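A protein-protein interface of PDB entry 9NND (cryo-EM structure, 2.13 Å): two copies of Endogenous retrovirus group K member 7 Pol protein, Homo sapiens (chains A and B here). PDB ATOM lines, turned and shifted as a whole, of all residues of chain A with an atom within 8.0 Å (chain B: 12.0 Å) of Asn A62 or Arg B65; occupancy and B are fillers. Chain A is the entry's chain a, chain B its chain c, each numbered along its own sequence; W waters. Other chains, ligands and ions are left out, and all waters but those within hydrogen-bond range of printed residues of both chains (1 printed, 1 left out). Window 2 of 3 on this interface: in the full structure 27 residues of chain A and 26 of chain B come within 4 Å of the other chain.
Among the printed residues, merely in contact across the chains: Phe A1 with Val B68, Ala A58 with Ile B69, Phe A1 with Ile B69, Leu A64 with Val B68, Asn A62 with Arg B65, Thr A67 with Val B68 and Leu A64 with Arg B65.
Ile A61 touches Arg B65, but with the chains exchanged Arg A65 does not touch Ile B61 (12.9 Å).
Asn A62 touches Arg B65, but with the chains exchanged Arg A65 does not touch Asn B62 (10.6 Å).
Leu A64 touches Arg B65, but with the chains exchanged Arg A65 does not touch Leu B64 (8.8 Å).
O of Ile A61 is in hydrogen-bond range of NE of Arg B65 (2.8 Å).
Hydrophobic or aromatic side chains of chain B within 4 Å of the printed part of chain A: Val B68 and Ile B69.
Among the printed residues, no Asp or Glu carboxylate lies within 4 Å of a Lys or Arg side-chain nitrogen of the other chain.
Asn A62 touches just one residue of chain B: Arg B65.
Of the printed residues of chain A, Arg B65 touches Ile A61 (2.8 Å), Asn A62 (3.8 Å) and Leu A64 (3.99 Å).
Of chain B, only Arg B65 (2.8 Å) comes within 4 Å of Ile A61.
Of the printed residues of chain A, Ile B69 touches Phe A1 (3.8 Å) and Ala A58 (3.7 Å).
Printed residues of chain B within 4 Å of Thr A67: Val B68 (3.9 Å).
Printed residues of chain A within 4 Å of Val B68: Phe A1, Leu A64 and Thr A67.
Printed residues of chain B within 4 Å of Ala A58: Ile B69 (3.7 Å).
Gln B66 touches none of the printed residues of chain A.
The nearest printed residue of chain A that does not touch Arg B65 is Asn A59 (4.3 Å).
The nearest printed residue of chain B that does not touch Phe A1 is Gly B72 (4.2 Å).
The backbone carbonyl oxygen (O) of Gln A60 lies close to the side-chain amide oxygen (OD1) of Asn A62.
The guanidinium group (NH1) of Arg B65 is in salt-bridge range of the side-chain carboxylate (OD1) of Asp B63.
Water W1 lies within hydrogen-bond range of O of Gly B72 and N of Phe A1.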
ATOM      1  N   PHE A   1      12.451 -27.405 -32.681  1.00  0.00           N
ATOM      2  CA  PHE A   1      13.319 -27.997 -33.689  1.00  0.00           C
ATOM      3  C   PHE A   1      13.423 -29.504 -33.495  1.00  0.00           C
ATOM      4  O   PHE A   1      13.935 -30.219 -34.354  1.00  0.00           O
ATOM      5  CB  PHE A   1      14.710 -27.361 -33.644  1.00  0.00           C
ATOM      6  CG  PHE A   1      15.226 -27.125 -32.255  1.00  0.00           C
ATOM      7  CD1 PHE A   1      15.813 -28.153 -31.534  1.00  0.00           C
ATOM      8  CD2 PHE A   1      15.132 -25.872 -31.670  1.00  0.00           C
ATOM      9  CE1 PHE A   1      16.292 -27.936 -30.258  1.00  0.00           C
ATOM     10  CE2 PHE A   1      15.611 -25.652 -30.393  1.00  0.00           C
ATOM     11  CZ  PHE A   1      16.190 -26.685 -29.687  1.00  0.00           C
ATOM     12  N   LEU A  57      14.614 -34.861 -25.336  1.00  0.00           N
ATOM     13  CA  LEU A  57      15.574 -34.895 -26.431  1.00  0.00           C
ATOM     14  C   LEU A  57      16.361 -33.596 -26.556  1.00  0.00           C
ATOM     15  O   LEU A  57      17.561 -33.628 -26.842  1.00  0.00           O
ATOM     16  CB  LEU A  57      14.856 -35.186 -27.750  1.00  0.00           C
ATOM     17  CG  LEU A  57      14.049 -36.482 -27.809  1.00  0.00           C
ATOM     18  CD1 LEU A  57      13.259 -36.565 -29.103  1.00  0.00           C
ATOM     19  CD2 LEU A  57      14.963 -37.679 -27.648  1.00  0.00           C
ATOM     20  N   ALA A  58      15.703 -32.453 -26.349  1.00  0.00           N
ATOM     21  CA  ALA A  58      16.355 -31.167 -26.579  1.00  0.00           C
ATOM     22  C   ALA A  58      17.503 -30.932 -25.605  1.00  0.00           C
ATOM     23  O   ALA A  58      18.561 -30.431 -25.998  1.00  0.00           O
ATOM     24  CB  ALA A  58      15.334 -30.035 -26.483  1.00  0.00           C
ATOM     25  N   ASN A  59      17.319 -31.288 -24.332  1.00  0.00           N
ATOM     26  CA  ASN A  59      18.327 -30.951 -23.331  1.00  0.00           C
ATOM     27  C   ASN A  59      19.613 -31.755 -23.480  1.00  0.00           C
ATOM     28  O   ASN A  59      20.599 -31.429 -22.812  1.00  0.00           O
ATOM     29  CB  ASN A  59      17.761 -31.113 -21.910  1.00  0.00           C
ATOM     30  CG  ASN A  59      17.287 -32.527 -21.606  1.00  0.00           C
ATOM     31  OD1 ASN A  59      17.646 -33.487 -22.285  1.00  0.00           O
ATOM     32  ND2 ASN A  59      16.474 -32.655 -20.566  1.00  0.00           N
ATOM     33  N   GLN A  60      19.634 -32.778 -24.332  1.00  0.00           N
ATOM     34  CA  GLN A  60      20.831 -33.579 -24.554  1.00  0.00           C
ATOM     35  C   GLN A  60      21.682 -33.084 -25.717  1.00  0.00           C
ATOM     36  O   GLN A  60      22.749 -33.655 -25.966  1.00  0.00           O
ATOM     37  CB  GLN A  60      20.449 -35.043 -24.798  1.00  0.00           C
ATOM     38  CG  GLN A  60      19.563 -35.647 -23.725  1.00  0.00           C
ATOM     39  CD  GLN A  60      19.374 -37.140 -23.901  1.00  0.00           C
ATOM     40  OE1 GLN A  60      20.291 -37.923 -23.666  1.00  0.00           O
ATOM     41  NE2 GLN A  60      18.182 -37.540 -24.316  1.00  0.00           N
ATOM     42  N   ILE A  61      21.249 -32.046 -26.430  1.00  0.00           N
ATOM     43  CA  ILE A  61      21.988 -31.580 -27.599  1.00  0.00           C
ATOM     44  C   ILE A  61      23.303 -30.957 -27.158  1.00  0.00           C
ATOM     45  O   ILE A  61      23.327 -30.031 -26.337  1.00  0.00           O
ATOM     46  CB  ILE A  61      21.145 -30.582 -28.406  1.00  0.00           C
ATOM     47  CG1 ILE A  61      19.906 -31.270 -28.979  1.00  0.00           C
ATOM     48  CG2 ILE A  61      21.972 -29.968 -29.522  1.00  0.00           C
ATOM     49  CD1 ILE A  61      18.880 -30.311 -29.530  1.00  0.00           C
ATOM     50  N   ASN A  62      24.408 -31.460 -27.707  1.00  0.00           N
ATOM     51  CA  ASN A  62      25.732 -30.918 -27.422  1.00  0.00           C
ATOM     52  C   ASN A  62      26.138 -29.879 -28.463  1.00  0.00           C
ATOM     53  O   ASN A  62      26.489 -28.747 -28.120  1.00  0.00           O
ATOM     54  CB  ASN A  62      26.765 -32.049 -27.363  1.00  0.00           C
ATOM     55  CG  ASN A  62      26.443 -33.079 -26.303  1.00  0.00           C
ATOM     56  OD1 ASN A  62      25.992 -32.739 -25.210  1.00  0.00           O
ATOM     57  ND2 ASN A  62      26.671 -34.347 -26.623  1.00  0.00           N
ATOM     58  N   ASP A  63      26.093 -30.256 -29.735  1.00  0.00           N
ATOM     59  CA  ASP A  63      26.439 -29.367 -30.837  1.00  0.00           C
ATOM     60  C   ASP A  63      25.170 -28.672 -31.315  1.00  0.00           C
ATOM     61  O   ASP A  63      24.297 -29.306 -31.917  1.00  0.00           O
ATOM     62  CB  ASP A  63      27.096 -30.158 -31.965  1.00  0.00           C
ATOM     63  CG  ASP A  63      27.766 -29.272 -32.989  1.00  0.00           C
ATOM     64  OD1 ASP A  63      27.405 -28.082 -33.082  1.00  0.00           O
ATOM     65  OD2 ASP A  63      28.659 -29.768 -33.703  1.00  0.00           O
ATOM     66  N   LEU A  64      25.073 -27.371 -31.064  1.00  0.00           N
ATOM     67  CA  LEU A  64      23.896 -26.595 -31.434  1.00  0.00           C
ATOM     68  C   LEU A  64      23.991 -25.989 -32.827  1.00  0.00           C
ATOM     69  O   LEU A  64      23.079 -25.261 -33.226  1.00  0.00           O
ATOM     70  CB  LEU A  64      23.656 -25.478 -30.411  1.00  0.00           C
ATOM     71  CG  LEU A  64      23.052 -25.860 -29.059  1.00  0.00           C
ATOM     72  CD1 LEU A  64      23.370 -24.797 -28.020  1.00  0.00           C
ATOM     73  CD2 LEU A  64      21.547 -26.074 -29.170  1.00  0.00           C
ATOM     74  N   ARG A  65      25.066 -26.264 -33.571  1.00  0.00           N
ATOM     75  CA  ARG A  65      25.278 -25.595 -34.853  1.00  0.00           C
ATOM     76  C   ARG A  65      24.182 -25.944 -35.859  1.00  0.00           C
ATOM     77  O   ARG A  65      23.591 -25.054 -36.483  1.00  0.00           O
ATOM     78  CB  ARG A  65      26.661 -25.952 -35.402  1.00  0.00           C
ATOM     79  CG  ARG A  65      27.781 -25.067 -34.868  1.00  0.00           C
ATOM     80  CD  ARG A  65      29.165 -25.642 -35.147  1.00  0.00           C
ATOM     81  NE  ARG A  65      30.137 -25.272 -34.124  1.00  0.00           N
ATOM     82  CZ  ARG A  65      30.473 -26.021 -33.082  1.00  0.00           C
ATOM     83  NH1 ARG A  65      29.978 -27.234 -32.914  1.00  0.00           N
ATOM     84  NH2 ARG A  65      31.342 -25.548 -32.195  1.00  0.00           N
ATOM     85  N   THR A  67      21.182 -27.155 -35.264  1.00  0.00           N
ATOM     86  CA  THR A  67      19.911 -26.634 -34.775  1.00  0.00           C
ATOM     87  C   THR A  67      19.799 -25.134 -35.019  1.00  0.00           C
ATOM     88  O   THR A  67      18.751 -24.647 -35.453  1.00  0.00           O
ATOM     89  CB  THR A  67      19.756 -26.949 -33.285  1.00  0.00           C
ATOM     90  OG1 THR A  67      19.504 -28.348 -33.116  1.00  0.00           O
ATOM     91  CG2 THR A  67      18.609 -26.154 -32.678  1.00  0.00           C
ATOM     92  N   PHE B   1      15.643 -12.723 -25.846  1.00  0.00           N
ATOM     93  CA  PHE B   1      15.399 -13.759 -24.853  1.00  0.00           C
ATOM     94  C   PHE B   1      15.808 -13.285 -23.464  1.00  0.00           C
ATOM     95  O   PHE B   1      15.508 -13.933 -22.463  1.00  0.00           O
ATOM     96  CB  PHE B   1      16.151 -15.042 -25.216  1.00  0.00           C
ATOM     97  CG  PHE B   1      17.541 -14.805 -25.733  1.00  0.00           C
ATOM     98  CD1 PHE B   1      18.592 -14.583 -24.858  1.00  0.00           C
ATOM     99  CD2 PHE B   1      17.799 -14.809 -27.093  1.00  0.00           C
ATOM    100  CE1 PHE B   1      19.871 -14.367 -25.330  1.00  0.00           C
ATOM    101  CE2 PHE B   1      19.080 -14.595 -27.569  1.00  0.00           C
ATOM    102  CZ  PHE B   1      20.115 -14.373 -26.685  1.00  0.00           C
ATOM    103  N   ALA B  58      23.281 -10.561 -22.170  1.00  0.00           N
ATOM    104  CA  ALA B  58      23.298 -11.574 -23.220  1.00  0.00           C
ATOM    105  C   ALA B  58      24.711 -12.054 -23.524  1.00  0.00           C
ATOM    106  O   ALA B  58      24.931 -13.256 -23.710  1.00  0.00           O
ATOM    107  CB  ALA B  58      22.637 -11.031 -24.486  1.00  0.00           C
ATOM    108  N   GLN B  60      27.189 -12.544 -21.747  1.00  0.00           N
ATOM    109  CA  GLN B  60      27.783 -13.376 -20.709  1.00  0.00           C
ATOM    110  C   GLN B  60      27.253 -14.805 -20.702  1.00  0.00           C
ATOM    111  O   GLN B  60      27.724 -15.617 -19.901  1.00  0.00           O
ATOM    112  CB  GLN B  60      27.550 -12.752 -19.330  1.00  0.00           C
ATOM    113  CG  GLN B  60      27.973 -11.301 -19.219  1.00  0.00           C
ATOM    114  CD  GLN B  60      27.881 -10.779 -17.800  1.00  0.00           C
ATOM    115  OE1 GLN B  60      28.721 -11.088 -16.958  1.00  0.00           O
ATOM    116  NE2 GLN B  60      26.856  -9.987 -17.528  1.00  0.00           N
ATOM    117  N   ILE B  61      26.295 -15.134 -21.568  1.00  0.00           N
ATOM    118  CA  ILE B  61      25.710 -16.470 -21.562  1.00  0.00           C
ATOM    119  C   ILE B  61      26.743 -17.482 -22.036  1.00  0.00           C
ATOM    120  O   ILE B  61      27.321 -17.343 -23.122  1.00  0.00           O
ATOM    121  CB  ILE B  61      24.450 -16.511 -22.438  1.00  0.00           C
ATOM    122  CG1 ILE B  61      23.368 -15.598 -21.861  1.00  0.00           C
ATOM    123  CG2 ILE B  61      23.934 -17.934 -22.561  1.00  0.00           C
ATOM    124  CD1 ILE B  61      22.277 -15.253 -22.844  1.00  0.00           C
ATOM    125  N   ASN B  62      26.982 -18.508 -21.221  1.00  0.00           N
ATOM    126  CA  ASN B  62      27.914 -19.575 -21.571  1.00  0.00           C
ATOM    127  C   ASN B  62      27.189 -20.755 -22.213  1.00  0.00           C
ATOM    128  O   ASN B  62      27.507 -21.155 -23.337  1.00  0.00           O
ATOM    129  CB  ASN B  62      28.687 -20.029 -20.328  1.00  0.00           C
ATOM    130  CG  ASN B  62      29.565 -18.935 -19.753  1.00  0.00           C
ATOM    131  OD1 ASN B  62      30.129 -18.124 -20.488  1.00  0.00           O
ATOM    132  ND2 ASN B  62      29.684 -18.908 -18.431  1.00  0.00           N
ATOM    133  N   ASP B  63      26.216 -21.319 -21.506  1.00  0.00           N
ATOM    134  CA  ASP B  63      25.418 -22.436 -22.002  1.00  0.00           C
ATOM    135  C   ASP B  63      24.205 -21.872 -22.732  1.00  0.00           C
ATOM    136  O   ASP B  63      23.312 -21.292 -22.107  1.00  0.00           O
ATOM    137  CB  ASP B  63      24.997 -23.338 -20.843  1.00  0.00           C
ATOM    138  CG  ASP B  63      24.459 -24.679 -21.303  1.00  0.00           C
ATOM    139  OD1 ASP B  63      23.911 -24.764 -22.420  1.00  0.00           O
ATOM    140  OD2 ASP B  63      24.587 -25.655 -20.538  1.00  0.00           O
ATOM    141  N   LEU B  64      24.169 -22.044 -24.049  1.00  0.00           N
ATOM    142  CA  LEU B  64      23.093 -21.506 -24.872  1.00  0.00           C
ATOM    143  C   LEU B  64      21.932 -22.475 -25.053  1.00  0.00           C
ATOM    144  O   LEU B  64      20.974 -22.136 -25.751  1.00  0.00           O
ATOM    145  CB  LEU B  64      23.632 -21.103 -26.249  1.00  0.00           C
ATOM    146  CG  LEU B  64      24.405 -19.788 -26.352  1.00  0.00           C
ATOM    147  CD1 LEU B  64      25.307 -19.809 -27.574  1.00  0.00           C
ATOM    148  CD2 LEU B  64      23.457 -18.596 -26.397  1.00  0.00           C
ATOM    149  N   ARG B  65      21.993 -23.663 -24.447  1.00  0.00           N
ATOM    150  CA  ARG B  65      20.982 -24.686 -24.702  1.00  0.00           C
ATOM    151  C   ARG B  65      19.589 -24.206 -24.310  1.00  0.00           C
ATOM    152  O   ARG B  65      18.642 -24.297 -25.101  1.00  0.00           O
ATOM    153  CB  ARG B  65      21.340 -25.971 -23.953  1.00  0.00           C
ATOM    154  CG  ARG B  65      22.418 -26.803 -24.631  1.00  0.00           C
ATOM    155  CD  ARG B  65      22.909 -27.919 -23.722  1.00  0.00           C
ATOM    156  NE  ARG B  65      24.173 -28.485 -24.176  1.00  0.00           N
ATOM    157  CZ  ARG B  65      25.372 -28.051 -23.814  1.00  0.00           C
ATOM    158  NH1 ARG B  65      25.517 -27.037 -22.979  1.00  0.00           N
ATOM    159  NH2 ARG B  65      26.454 -28.654 -24.298  1.00  0.00           N
ATOM    160  N   GLN B  66      19.446 -23.679 -23.092  1.00  0.00           N
ATOM    161  CA  GLN B  66      18.137 -23.221 -22.633  1.00  0.00           C
ATOM    162  C   GLN B  66      17.623 -22.066 -23.485  1.00  0.00           C
ATOM    163  O   GLN B  66      16.435 -22.013 -23.822  1.00  0.00           O
ATOM    164  CB  GLN B  66      18.208 -22.815 -21.161  1.00  0.00           C
ATOM    165  CG  GLN B  66      16.875 -22.376 -20.573  1.00  0.00           C
ATOM    166  CD  GLN B  66      16.043 -23.541 -20.063  1.00  0.00           C
ATOM    167  OE1 GLN B  66      16.219 -24.679 -20.494  1.00  0.00           O
ATOM    168  NE2 GLN B  66      15.135 -23.260 -19.141  1.00  0.00           N
ATOM    169  N   THR B  67      18.509 -21.136 -23.847  1.00  0.00           N
ATOM    170  CA  THR B  67      18.117 -20.020 -24.699  1.00  0.00           C
ATOM    171  C   THR B  67      17.660 -20.506 -26.068  1.00  0.00           C
ATOM    172  O   THR B  67      16.650 -20.031 -26.598  1.00  0.00           O
ATOM    173  CB  THR B  67      19.280 -19.037 -24.842  1.00  0.00           C
ATOM    174  OG1 THR B  67      19.465 -18.330 -23.610  1.00  0.00           O
ATOM    175  CG2 THR B  67      19.011 -18.037 -25.958  1.00  0.00           C
ATOM    176  N   VAL B  68      18.383 -21.464 -26.651  1.00  0.00           N
ATOM    177  CA  VAL B  68      18.023 -21.960 -27.974  1.00  0.00           C
ATOM    178  C   VAL B  68      16.695 -22.707 -27.920  1.00  0.00           C
ATOM    179  O   VAL B  68      15.866 -22.581 -28.824  1.00  0.00           O
ATOM    180  CB  VAL B  68      19.156 -22.831 -28.547  1.00  0.00           C
ATOM    181  CG1 VAL B  68      18.672 -23.637 -29.741  1.00  0.00           C
ATOM    182  CG2 VAL B  68      20.337 -21.959 -28.944  1.00  0.00           C
ATOM    183  N   ILE B  69      16.464 -23.481 -26.857  1.00  0.00           N
ATOM    184  CA  ILE B  69      15.195 -24.194 -26.719  1.00  0.00           C
ATOM    185  C   ILE B  69      14.036 -23.214 -26.556  1.00  0.00           C
ATOM    186  O   ILE B  69      12.971 -23.378 -27.169  1.00  0.00           O
ATOM    187  CB  ILE B  69      15.271 -25.189 -25.546  1.00  0.00           C
ATOM    188  CG1 ILE B  69      16.201 -26.350 -25.901  1.00  0.00           C
ATOM    189  CG2 ILE B  69      13.885 -25.704 -25.179  1.00  0.00           C
ATOM    190  CD1 ILE B  69      16.692 -27.129 -24.706  1.00  0.00           C
ATOM    191  N   TRP B  70      14.222 -22.181 -25.729  1.00  0.00           N
ATOM    192  CA  TRP B  70      13.185 -21.168 -25.562  1.00  0.00           C
ATOM    193  C   TRP B  70      12.897 -20.453 -26.879  1.00  0.00           C
ATOM    194  O   TRP B  70      11.732 -20.243 -27.240  1.00  0.00           O
ATOM    195  CB  TRP B  70      13.609 -20.178 -24.477  1.00  0.00           C
ATOM    196  CG  TRP B  70      12.614 -19.102 -24.200  1.00  0.00           C
ATOM    197  CD1 TRP B  70      11.619 -19.126 -23.269  1.00  0.00           C
ATOM    198  CD2 TRP B  70      12.524 -17.832 -24.852  1.00  0.00           C
ATOM    199  NE1 TRP B  70      10.909 -17.952 -23.305  1.00  0.00           N
ATOM    200  CE2 TRP B  70      11.446 -17.139 -24.268  1.00  0.00           C
ATOM    201  CE3 TRP B  70      13.248 -17.213 -25.874  1.00  0.00           C
ATOM    202  CZ2 TRP B  70      11.074 -15.859 -24.673  1.00  0.00           C
ATOM    203  CZ3 TRP B  70      12.878 -15.942 -26.274  1.00  0.00           C
ATOM    204  CH2 TRP B  70      11.801 -15.279 -25.675  1.00  0.00           C
ATOM    205  N   MET B  71      13.948 -20.094 -27.620  1.00  0.00           N
ATOM    206  CA  MET B  71      13.757 -19.445 -28.912  1.00  0.00           C
ATOM    207  C   MET B  71      13.063 -20.371 -29.901  1.00  0.00           C
ATOM    208  O   MET B  71      12.258 -19.920 -30.718  1.00  0.00           O
ATOM    209  CB  MET B  71      15.099 -18.980 -29.476  1.00  0.00           C
ATOM    210  CG  MET B  71      15.751 -17.842 -28.714  1.00  0.00           C
ATOM    211  SD  MET B  71      17.359 -17.413 -29.406  1.00  0.00           S
ATOM    212  CE  MET B  71      16.936 -17.208 -31.133  1.00  0.00           C
ATOM    213  N   GLY B  72      13.381 -21.665 -29.858  1.00  0.00           N
ATOM    214  CA  GLY B  72      12.721 -22.609 -30.743  1.00  0.00           C
ATOM    215  C   GLY B  72      11.242 -22.735 -30.448  1.00  0.00           C
ATOM    216  O   GLY B  72      10.419 -22.787 -31.364  1.00  0.00           O
ATOM    217  N   ASP B  73      10.883 -22.775 -29.164  1.00  0.00           N
ATOM    218  CA  ASP B  73       9.466 -22.787 -28.814  1.00  0.00           C
ATOM    219  C   ASP B  73       8.783 -21.506 -29.278  1.00  0.00           C
ATOM    220  O   ASP B  73       7.669 -21.548 -29.814  1.00  0.00           O
ATOM    221  CB  ASP B  73       9.283 -22.974 -27.310  1.00  0.00           C
ATOM    222  CG  ASP B  73       7.872 -22.653 -26.855  1.00  0.00           C
ATOM    223  OD1 ASP B  73       6.993 -23.531 -26.977  1.00  0.00           O
ATOM    224  OD2 ASP B  73       7.634 -21.521 -26.382  1.00  0.00           O
ATOM    225  N   ARG B  74       9.441 -20.358 -29.090  1.00  0.00           N
ATOM    226  CA  ARG B  74       8.862 -19.092 -29.537  1.00  0.00           C
ATOM    227  C   ARG B  74       8.669 -19.073 -31.049  1.00  0.00           C
ATOM    228  O   ARG B  74       7.630 -18.624 -31.543  1.00  0.00           O
ATOM    229  CB  ARG B  74       9.743 -17.924 -29.095  1.00  0.00           C
ATOM    230  CG  ARG B  74       9.797 -17.716 -27.590  1.00  0.00           C
ATOM    231  CD  ARG B  74       8.502 -17.125 -27.063  1.00  0.00           C
ATOM    232  NE  ARG B  74       8.479 -15.674 -27.195  1.00  0.00           N
ATOM    233  CZ  ARG B  74       8.087 -14.839 -26.244  1.00  0.00           C
ATOM    234  NH1 ARG B  74       7.671 -15.277 -25.067  1.00  0.00           N
ATOM    235  NH2 ARG B  74       8.112 -13.530 -26.479  1.00  0.00           N
HETATM  236  O   HOH W   1      11.336 -24.653 -33.375  1.00  0.00           O
